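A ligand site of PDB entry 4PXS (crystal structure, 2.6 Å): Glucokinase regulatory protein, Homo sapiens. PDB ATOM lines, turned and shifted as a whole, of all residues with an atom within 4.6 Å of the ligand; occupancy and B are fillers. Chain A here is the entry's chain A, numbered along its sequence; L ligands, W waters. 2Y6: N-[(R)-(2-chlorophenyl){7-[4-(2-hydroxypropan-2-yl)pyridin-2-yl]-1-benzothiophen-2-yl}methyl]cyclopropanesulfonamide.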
ATOM      1  N   HIS A  21      18.275  17.577  16.461  1.00  0.00           N
ATOM      2  CA  HIS A  21      17.380  18.517  17.121  1.00  0.00           C
ATOM      3  C   HIS A  21      15.902  18.137  17.315  1.00  0.00           C
ATOM      4  O   HIS A  21      15.180  18.890  17.954  1.00  0.00           O
ATOM      5  CB  HIS A  21      17.424  19.849  16.358  1.00  0.00           C
ATOM      6  CG  HIS A  21      17.110  19.717  14.898  1.00  0.00           C
ATOM      7  ND1 HIS A  21      16.307  20.612  14.236  1.00  0.00           N
ATOM      8  CD2 HIS A  21      17.483  18.784  13.978  1.00  0.00           C
ATOM      9  CE1 HIS A  21      16.201  20.240  12.971  1.00  0.00           C
ATOM     10  NE2 HIS A  21      16.908  19.141  12.793  1.00  0.00           N
ATOM     11  N   VAL A  22      15.416  17.031  16.781  1.00  0.00           N
ATOM     12  CA  VAL A  22      14.026  16.664  17.058  1.00  0.00           C
ATOM     13  C   VAL A  22      13.939  16.139  18.484  1.00  0.00           C
ATOM     14  O   VAL A  22      14.779  15.310  18.909  1.00  0.00           O
ATOM     15  CB  VAL A  22      13.521  15.590  16.099  1.00  0.00           C
ATOM     16  CG1 VAL A  22      12.128  15.147  16.503  1.00  0.00           C
ATOM     17  CG2 VAL A  22      13.536  16.106  14.681  1.00  0.00           C
ATOM     18  N   ILE A  23      12.961  16.618  19.254  1.00  0.00           N
ATOM     19  CA  ILE A  23      12.875  16.185  20.637  1.00  0.00           C
ATOM     20  C   ILE A  23      12.361  14.759  20.662  1.00  0.00           C
ATOM     21  O   ILE A  23      11.488  14.378  19.882  1.00  0.00           O
ATOM     22  CB  ILE A  23      11.983  17.055  21.534  1.00  0.00           C
ATOM     23  CG1 ILE A  23      12.262  18.578  21.363  1.00  0.00           C
ATOM     24  CG2 ILE A  23      12.179  16.650  22.988  1.00  0.00           C
ATOM     25  CD1 ILE A  23      13.675  19.022  21.677  1.00  0.00           C
ATOM     26  N   TYR A  36       8.700  18.450  27.590  1.00  0.00           N
ATOM     27  CA  TYR A  36       8.381  18.480  26.186  1.00  0.00           C
ATOM     28  C   TYR A  36       7.228  19.473  25.948  1.00  0.00           C
ATOM     29  O   TYR A  36       7.361  20.411  25.172  1.00  0.00           O
ATOM     30  CB  TYR A  36       8.089  17.044  25.690  1.00  0.00           C
ATOM     31  CG  TYR A  36       7.790  16.855  24.217  1.00  0.00           C
ATOM     32  CD1 TYR A  36       6.612  17.304  23.686  1.00  0.00           C
ATOM     33  CD2 TYR A  36       8.662  16.198  23.380  1.00  0.00           C
ATOM     34  CE1 TYR A  36       6.309  17.134  22.364  1.00  0.00           C
ATOM     35  CE2 TYR A  36       8.360  16.033  22.044  1.00  0.00           C
ATOM     36  CZ  TYR A  36       7.163  16.499  21.538  1.00  0.00           C
ATOM     37  OH  TYR A  36       6.770  16.339  20.212  1.00  0.00           O
ATOM     38  N   ALA A  39       8.242  22.861  25.477  1.00  0.00           N
ATOM     39  CA  ALA A  39       9.071  23.083  24.297  1.00  0.00           C
ATOM     40  C   ALA A  39       8.271  23.176  22.992  1.00  0.00           C
ATOM     41  O   ALA A  39       8.842  23.586  21.973  1.00  0.00           O
ATOM     42  CB  ALA A  39      10.084  21.949  24.167  1.00  0.00           C
ATOM     43  N   VAL A  40       7.000  22.771  23.012  1.00  0.00           N
ATOM     44  CA  VAL A  40       6.199  22.798  21.793  1.00  0.00           C
ATOM     45  C   VAL A  40       5.923  24.234  21.451  1.00  0.00           C
ATOM     46  O   VAL A  40       5.240  24.932  22.203  1.00  0.00           O
ATOM     47  CB  VAL A  40       4.829  22.071  21.900  1.00  0.00           C
ATOM     48  CG1 VAL A  40       4.124  22.087  20.545  1.00  0.00           C
ATOM     49  CG2 VAL A  40       4.979  20.655  22.406  1.00  0.00           C
ATOM     50  N   PRO A  41       6.393  24.682  20.296  1.00  0.00           N
ATOM     51  CA  PRO A  41       6.103  26.078  19.944  1.00  0.00           C
ATOM     52  C   PRO A  41       4.636  26.437  20.086  1.00  0.00           C
ATOM     53  O   PRO A  41       3.773  25.613  19.845  1.00  0.00           O
ATOM     54  CB  PRO A  41       6.578  26.171  18.487  1.00  0.00           C
ATOM     55  CG  PRO A  41       7.691  25.152  18.415  1.00  0.00           C
ATOM     56  CD  PRO A  41       7.172  24.007  19.251  1.00  0.00           C
ATOM     57  N   THR A  43       2.673  28.118  18.380  1.00  0.00           N
ATOM     58  CA  THR A  43       1.929  28.096  17.130  1.00  0.00           C
ATOM     59  C   THR A  43       1.590  26.720  16.705  1.00  0.00           C
ATOM     60  O   THR A  43       0.710  26.540  15.888  1.00  0.00           O
ATOM     61  CB  THR A  43       2.741  28.732  15.974  1.00  0.00           C
ATOM     62  OG1 THR A  43       3.973  28.029  15.772  1.00  0.00           O
ATOM     63  CG2 THR A  43       3.042  30.182  16.298  1.00  0.00           C
ATOM     64  N   GLU A  44       2.289  25.741  17.222  1.00  0.00           N
ATOM     65  CA  GLU A  44       2.048  24.363  16.854  1.00  0.00           C
ATOM     66  C   GLU A  44       1.241  23.624  17.897  1.00  0.00           C
ATOM     67  O   GLU A  44       0.857  22.473  17.665  1.00  0.00           O
ATOM     68  CB  GLU A  44       3.390  23.655  16.688  1.00  0.00           C
ATOM     69  CG  GLU A  44       4.155  24.120  15.470  1.00  0.00           C
ATOM     70  CD  GLU A  44       3.496  23.728  14.147  1.00  0.00           C
ATOM     71  OE1 GLU A  44       2.873  22.653  14.050  1.00  0.00           O
ATOM     72  OE2 GLU A  44       3.600  24.509  13.198  1.00  0.00           O
ATOM     73  N   SER A  46      -1.469  22.043  20.611  1.00  0.00           N
ATOM     74  CA  SER A  46      -2.825  21.571  20.776  1.00  0.00           C
ATOM     75  C   SER A  46      -3.469  22.531  21.743  1.00  0.00           C
ATOM     76  O   SER A  46      -3.050  22.587  22.898  1.00  0.00           O
ATOM     77  CB  SER A  46      -2.819  20.159  21.376  1.00  0.00           C
ATOM     78  OG  SER A  46      -4.104  19.827  21.874  1.00  0.00           O
ATOM     79  N   GLY A 193       4.929  31.576  12.828  1.00  0.00           N
ATOM     80  CA  GLY A 193       5.690  30.621  13.596  1.00  0.00           C
ATOM     81  C   GLY A 193       7.131  31.028  13.874  1.00  0.00           C
ATOM     82  O   GLY A 193       7.869  30.263  14.484  1.00  0.00           O
ATOM     83  N   SER A 195       9.173  31.069  11.431  1.00  0.00           N
ATOM     84  CA  SER A 195       9.472  29.812  10.737  1.00  0.00           C
ATOM     85  C   SER A 195      10.024  29.885   9.303  1.00  0.00           C
ATOM     86  O   SER A 195      10.936  29.140   8.958  1.00  0.00           O
ATOM     87  CB  SER A 195       8.182  28.999  10.638  1.00  0.00           C
ATOM     88  OG  SER A 195       8.332  28.008   9.628  1.00  0.00           O
ATOM     89  N   ASN A 221       5.417  33.353  18.272  1.00  0.00           N
ATOM     90  CA  ASN A 221       6.127  32.565  19.233  1.00  0.00           C
ATOM     91  C   ASN A 221       7.138  33.427  19.867  1.00  0.00           C
ATOM     92  O   ASN A 221       7.665  34.334  19.206  1.00  0.00           O
ATOM     93  CB  ASN A 221       6.841  31.432  18.563  1.00  0.00           C
ATOM     94  CG  ASN A 221       5.917  30.275  18.241  1.00  0.00           C
ATOM     95  OD1 ASN A 221       5.044  29.950  19.019  1.00  0.00           O
ATOM     96  ND2 ASN A 221       6.113  29.652  17.072  1.00  0.00           N
ATOM     97  N   MET A 225      11.289  29.956  21.029  1.00  0.00           N
ATOM     98  CA  MET A 225      10.636  28.834  20.333  1.00  0.00           C
ATOM     99  C   MET A 225      10.790  28.913  18.821  1.00  0.00           C
ATOM    100  O   MET A 225      10.413  28.005  18.110  1.00  0.00           O
ATOM    101  CB  MET A 225       9.164  28.752  20.677  1.00  0.00           C
ATOM    102  CG  MET A 225       8.930  28.265  22.094  1.00  0.00           C
ATOM    103  SD  MET A 225       7.255  28.644  22.659  1.00  0.00           S
ATOM    104  CE  MET A 225       7.202  27.710  24.173  1.00  0.00           C
ATOM    105  N   ALA A 226      11.349  29.996  18.323  1.00  0.00           N
ATOM    106  CA  ALA A 226      11.606  30.144  16.931  1.00  0.00           C
ATOM    107  C   ALA A 226      12.307  28.918  16.339  1.00  0.00           C
ATOM    108  O   ALA A 226      13.201  28.304  16.962  1.00  0.00           O
ATOM    109  CB  ALA A 226      12.452  31.385  16.706  1.00  0.00           C
ATOM    110  N   ARG A 227      11.889  28.570  15.125  1.00  0.00           N
ATOM    111  CA  ARG A 227      12.471  27.481  14.362  1.00  0.00           C
ATOM    112  C   ARG A 227      13.998  27.571  14.418  1.00  0.00           C
ATOM    113  O   ARG A 227      14.617  28.632  14.095  1.00  0.00           O
ATOM    114  CB  ARG A 227      12.015  27.531  12.902  1.00  0.00           C
ATOM    115  CG  ARG A 227      11.455  26.241  12.454  1.00  0.00           C
ATOM    116  CD  ARG A 227      10.826  26.303  11.095  1.00  0.00           C
ATOM    117  NE  ARG A 227      11.205  25.109  10.328  1.00  0.00           N
ATOM    118  CZ  ARG A 227      10.880  24.857   9.079  1.00  0.00           C
ATOM    119  NH1 ARG A 227      10.112  25.692   8.381  1.00  0.00           N
ATOM    120  NH2 ARG A 227      11.310  23.748   8.505  1.00  0.00           N
ATOM    121  N   ASN A 228      14.573  26.439  14.865  1.00  0.00           N
ATOM    122  CA  ASN A 228      15.987  26.200  14.874  1.00  0.00           C
ATOM    123  C   ASN A 228      16.437  25.192  13.845  1.00  0.00           C
ATOM    124  O   ASN A 228      17.509  24.636  14.013  1.00  0.00           O
ATOM    125  CB  ASN A 228      16.452  25.742  16.260  1.00  0.00           C
ATOM    126  CG  ASN A 228      17.832  26.274  16.617  1.00  0.00           C
ATOM    127  OD1 ASN A 228      18.288  27.336  16.122  1.00  0.00           O
ATOM    128  ND2 ASN A 228      18.533  25.539  17.466  1.00  0.00           N
ATOM    129  N   ASP A 229      15.703  24.942  12.765  1.00  0.00           N
ATOM    130  CA  ASP A 229      16.221  23.948  11.832  1.00  0.00           C
ATOM    131  C   ASP A 229      17.161  24.509  10.775  1.00  0.00           C
ATOM    132  O   ASP A 229      17.008  25.631  10.326  1.00  0.00           O
ATOM    133  CB  ASP A 229      15.156  22.979  11.262  1.00  0.00           C
ATOM    134  CG  ASP A 229      14.318  23.583  10.238  1.00  0.00           C
ATOM    135  OD1 ASP A 229      14.206  24.819  10.267  1.00  0.00           O
ATOM    136  OD2 ASP A 229      13.748  22.809   9.416  1.00  0.00           O
ATOM    137  N   HIS A 516      -6.132  17.931  15.451  1.00  0.00           N
ATOM    138  CA  HIS A 516      -4.992  17.871  14.535  1.00  0.00           C
ATOM    139  C   HIS A 516      -5.471  17.447  13.158  1.00  0.00           C
ATOM    140  O   HIS A 516      -6.369  16.617  13.038  1.00  0.00           O
ATOM    141  CB  HIS A 516      -3.954  16.843  15.005  1.00  0.00           C
ATOM    142  CG  HIS A 516      -3.404  17.074  16.367  1.00  0.00           C
ATOM    143  ND1 HIS A 516      -2.571  18.126  16.671  1.00  0.00           N
ATOM    144  CD2 HIS A 516      -3.510  16.352  17.514  1.00  0.00           C
ATOM    145  CE1 HIS A 516      -2.219  18.070  17.939  1.00  0.00           C
ATOM    146  NE2 HIS A 516      -2.769  16.985  18.473  1.00  0.00           N
ATOM    147  N   LYS A 526       8.493  22.626   7.108  1.00  0.00           N
ATOM    148  CA  LYS A 526       7.631  22.766   8.319  1.00  0.00           C
ATOM    149  C   LYS A 526       6.611  21.644   8.431  1.00  0.00           C
ATOM    150  O   LYS A 526       6.400  21.036   9.490  1.00  0.00           O
ATOM    151  CB  LYS A 526       6.900  24.114   8.282  1.00  0.00           C
ATOM    152  CG  LYS A 526       5.921  24.355   9.401  1.00  0.00           C
ATOM    153  CD  LYS A 526       5.560  25.841   9.520  1.00  0.00           C
ATOM    154  CE  LYS A 526       4.470  26.277   8.553  1.00  0.00           C
ATOM    155  NZ  LYS A 526       4.265  27.737   8.741  1.00  0.00           N
ATOM    156  N   TRP A 529       7.996  18.505   9.441  1.00  0.00           N
ATOM    157  CA  TRP A 529       8.251  18.352  10.860  1.00  0.00           C
ATOM    158  C   TRP A 529       6.940  18.159  11.626  1.00  0.00           C
ATOM    159  O   TRP A 529       6.895  17.357  12.552  1.00  0.00           O
ATOM    160  CB  TRP A 529       9.010  19.550  11.393  1.00  0.00           C
ATOM    161  CG  TRP A 529      10.389  19.705  10.835  1.00  0.00           C
ATOM    162  CD1 TRP A 529      10.903  20.808  10.244  1.00  0.00           C
ATOM    163  CD2 TRP A 529      11.442  18.729  10.843  1.00  0.00           C
ATOM    164  NE1 TRP A 529      12.215  20.595   9.880  1.00  0.00           N
ATOM    165  CE2 TRP A 529      12.568  19.328  10.248  1.00  0.00           C
ATOM    166  CE3 TRP A 529      11.545  17.421  11.322  1.00  0.00           C
ATOM    167  CZ2 TRP A 529      13.772  18.659  10.096  1.00  0.00           C
ATOM    168  CZ3 TRP A 529      12.728  16.749  11.161  1.00  0.00           C
ATOM    169  CH2 TRP A 529      13.838  17.370  10.541  1.00  0.00           C
ATOM    170  N   ARG A 530       5.873  18.852  11.216  1.00  0.00           N
ATOM    171  CA  ARG A 530       4.564  18.622  11.841  1.00  0.00           C
ATOM    172  C   ARG A 530       4.165  17.162  11.676  1.00  0.00           C
ATOM    173  O   ARG A 530       3.771  16.489  12.625  1.00  0.00           O
ATOM    174  CB  ARG A 530       3.481  19.573  11.290  1.00  0.00           C
ATOM    175  CG  ARG A 530       2.095  19.504  11.973  1.00  0.00           C
ATOM    176  CD  ARG A 530       1.165  20.601  11.485  1.00  0.00           C
ATOM    177  NE  ARG A 530       1.781  21.910  11.641  1.00  0.00           N
ATOM    178  CZ  ARG A 530       1.645  22.952  10.822  1.00  0.00           C
ATOM    179  NH1 ARG A 530       0.878  22.893   9.780  1.00  0.00           N
ATOM    180  NH2 ARG A 530       2.327  24.059  11.027  1.00  0.00           N
ATOM    181  N   ALA A 533       6.040  15.159  14.142  1.00  0.00           N
ATOM    182  CA  ALA A 533       5.602  15.382  15.528  1.00  0.00           C
ATOM    183  C   ALA A 533       4.245  14.745  15.791  1.00  0.00           C
ATOM    184  O   ALA A 533       3.984  14.253  16.898  1.00  0.00           O
ATOM    185  CB  ALA A 533       5.553  16.857  15.856  1.00  0.00           C
ATOM    186  N   MET A 534       3.393  14.746  14.773  1.00  0.00           N
ATOM    187  CA  MET A 534       2.088  14.072  14.906  1.00  0.00           C
ATOM    188  C   MET A 534       2.255  12.570  15.033  1.00  0.00           C
ATOM    189  O   MET A 534       1.540  11.945  15.833  1.00  0.00           O
ATOM    190  CB  MET A 534       1.154  14.389  13.751  1.00  0.00           C
ATOM    191  CG  MET A 534       0.658  15.808  13.807  1.00  0.00           C
ATOM    192  SD  MET A 534      -0.757  15.970  12.717  1.00  0.00           S
ATOM    193  CE  MET A 534       0.077  15.800  11.153  1.00  0.00           C
ATOM    194  N   ARG A 537       3.397  12.093  18.670  1.00  0.00           N
ATOM    195  CA  ARG A 537       2.257  12.326  19.541  1.00  0.00           C
ATOM    196  C   ARG A 537       1.222  11.197  19.518  1.00  0.00           C
ATOM    197  O   ARG A 537       0.709  10.759  20.541  1.00  0.00           O
ATOM    198  CB  ARG A 537       1.577  13.636  19.154  1.00  0.00           C
ATOM    199  CG  ARG A 537       0.303  13.989  19.923  1.00  0.00           C
ATOM    200  CD  ARG A 537       0.593  14.366  21.355  1.00  0.00           C
ATOM    201  NE  ARG A 537       1.343  15.610  21.490  1.00  0.00           N
ATOM    202  CZ  ARG A 537       1.607  16.192  22.651  1.00  0.00           C
ATOM    203  NH1 ARG A 537       1.218  15.649  23.802  1.00  0.00           N
ATOM    204  NH2 ARG A 537       2.289  17.323  22.679  1.00  0.00           N
HETATM  205 CL1  2Y6 L   1       7.733  23.084  12.576  1.00  0.00          CL
HETATM  206  C23 2Y6 L   1       8.089  24.402  13.638  1.00  0.00           C
HETATM  207  C22 2Y6 L   1       7.341  25.558  13.529  1.00  0.00           C
HETATM  208  C21 2Y6 L   1       7.564  26.662  14.337  1.00  0.00           C
HETATM  209  C20 2Y6 L   1       8.551  26.588  15.301  1.00  0.00           C
HETATM  210  C19 2Y6 L   1       9.288  25.426  15.437  1.00  0.00           C
HETATM  211  C18 2Y6 L   1       9.065  24.326  14.616  1.00  0.00           C
HETATM  212  C17 2Y6 L   1       9.921  23.083  14.820  1.00  0.00           C
HETATM  213  N2  2Y6 L   1      11.302  23.497  15.095  1.00  0.00           N
HETATM  214  S2  2Y6 L   1      12.323  22.750  14.099  1.00  0.00           S
HETATM  215  O2  2Y6 L   1      13.547  23.579  14.132  1.00  0.00           O
HETATM  216  O3  2Y6 L   1      11.773  22.607  12.708  1.00  0.00           O
HETATM  217  C24 2Y6 L   1      12.776  21.126  14.756  1.00  0.00           C
HETATM  218  C25 2Y6 L   1      11.575  20.225  14.962  1.00  0.00           C
HETATM  219  C26 2Y6 L   1      12.536  19.986  13.784  1.00  0.00           C
HETATM  220  C8  2Y6 L   1       9.317  22.301  15.954  1.00  0.00           C
HETATM  221  C7  2Y6 L   1       9.917  22.077  17.131  1.00  0.00           C
HETATM  222  S1  2Y6 L   1       7.733  21.593  15.926  1.00  0.00           S
HETATM  223  C5  2Y6 L   1       7.881  20.961  17.480  1.00  0.00           C
HETATM  224  C6  2Y6 L   1       9.148  21.350  18.004  1.00  0.00           C
HETATM  225  C3  2Y6 L   1       9.504  20.962  19.305  1.00  0.00           C
HETATM  226  C2  2Y6 L   1       8.617  20.202  20.036  1.00  0.00           C
HETATM  227  C1  2Y6 L   1       7.362  19.824  19.494  1.00  0.00           C
HETATM  228  C4  2Y6 L   1       7.002  20.186  18.208  1.00  0.00           C
HETATM  229  C9  2Y6 L   1       5.734  19.863  17.657  1.00  0.00           C
HETATM  230  C13 2Y6 L   1       4.734  19.189  18.410  1.00  0.00           C
HETATM  231  N1  2Y6 L   1       5.426  20.254  16.411  1.00  0.00           N
HETATM  232  C10 2Y6 L   1       4.243  19.992  15.904  1.00  0.00           C
HETATM  233  C11 2Y6 L   1       3.215  19.316  16.589  1.00  0.00           C
HETATM  234  C12 2Y6 L   1       3.468  18.898  17.875  1.00  0.00           C
HETATM  235  C14 2Y6 L   1       2.391  18.156  18.635  1.00  0.00           C
HETATM  236  C15 2Y6 L   1       1.576  17.374  17.626  1.00  0.00           C
HETATM  237  C16 2Y6 L   1       1.515  19.060  19.454  1.00  0.00           C
HETATM  238  O1  2Y6 L   1       2.977  17.325  19.554  1.00  0.00           O
HETATM  239  O   HOH W   1       4.759  15.415  19.054  1.00  0.00           O
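Water W1 lies within hydrogen-bond range of the side-chain hydroxyl of Tyr 36, the backbone carbonyl oxygen of Ala 533 and an oxygen (O1) of the ligand.
NE of Arg 227 sits at hydrogen-bond distance from O3 of the ligand, at 3.5 Å. The indole nitrogen of Trp 529 lies close to an oxygen (O3) of the ligand (3.5 Å). An oxygen (O1) of the ligand lies within hydrogen-bond range of the guanidinium group of Arg 537 (3.1 Å). An oxygen (O2) of the ligand sits at hydrogen-bond distance from the backbone NH (N) of Asp 229, 2.9 Å away. The backbone NH of Asn 228 lies within hydrogen-bond range of an oxygen (O2) of the ligand (3.1 Å).
The backbone carbonyl oxygen (O) of Gly 193 is in hydrogen-bond range of the side-chain amide nitrogen (ND2) of Asn 221, 3.2 Å away. OD2 of Asp 229 lies within hydrogen-bond range of NE1 of Trp 529, at 2.7 Å. The guanidinium group of Arg 227 is in salt-bridge range of the side-chain carboxylate of Asp 229 (2.8 Å). NH1 of Arg 227 lies within hydrogen-bond range of OG of Ser 195 (3.2 Å). The side-chain carboxylate (OE2) of Glu 44 is in salt-bridge range of the guanidinium group (NH2) of Arg 530, at 2.6 Å.
Residues that only touch the ligand: Pro 41 (3.4 Å), Ala 533 (3.4 Å), Glu 44 (3.5 Å), His 21 (3.6 Å), Tyr 36 (3.6 Å), Gly 193 (3.6 Å), Val 40 (3.7 Å), Met 225 (3.7 Å), Ala 39 (3.8 Å), Lys 526 (3.9 Å) and His 516 (3.9 Å). Hydrophobic or aromatic side chains that line the ligand: His 21, Tyr 36, Val 40, Pro 41, His 516, Trp 529 and Ala 533. 16 residues have an atom within 4 Å of the ligand: His 21, Tyr 36, Ala 39, Val 40, Pro 41, Glu 44, Gly 193, Met 225, Arg 227, Asn 228, Asp 229, His 516, Lys 526, Trp 529, Ala 533 and Arg 537. The nearest printed residue that does not touch the ligand is Thr 43 (4.1 Å).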
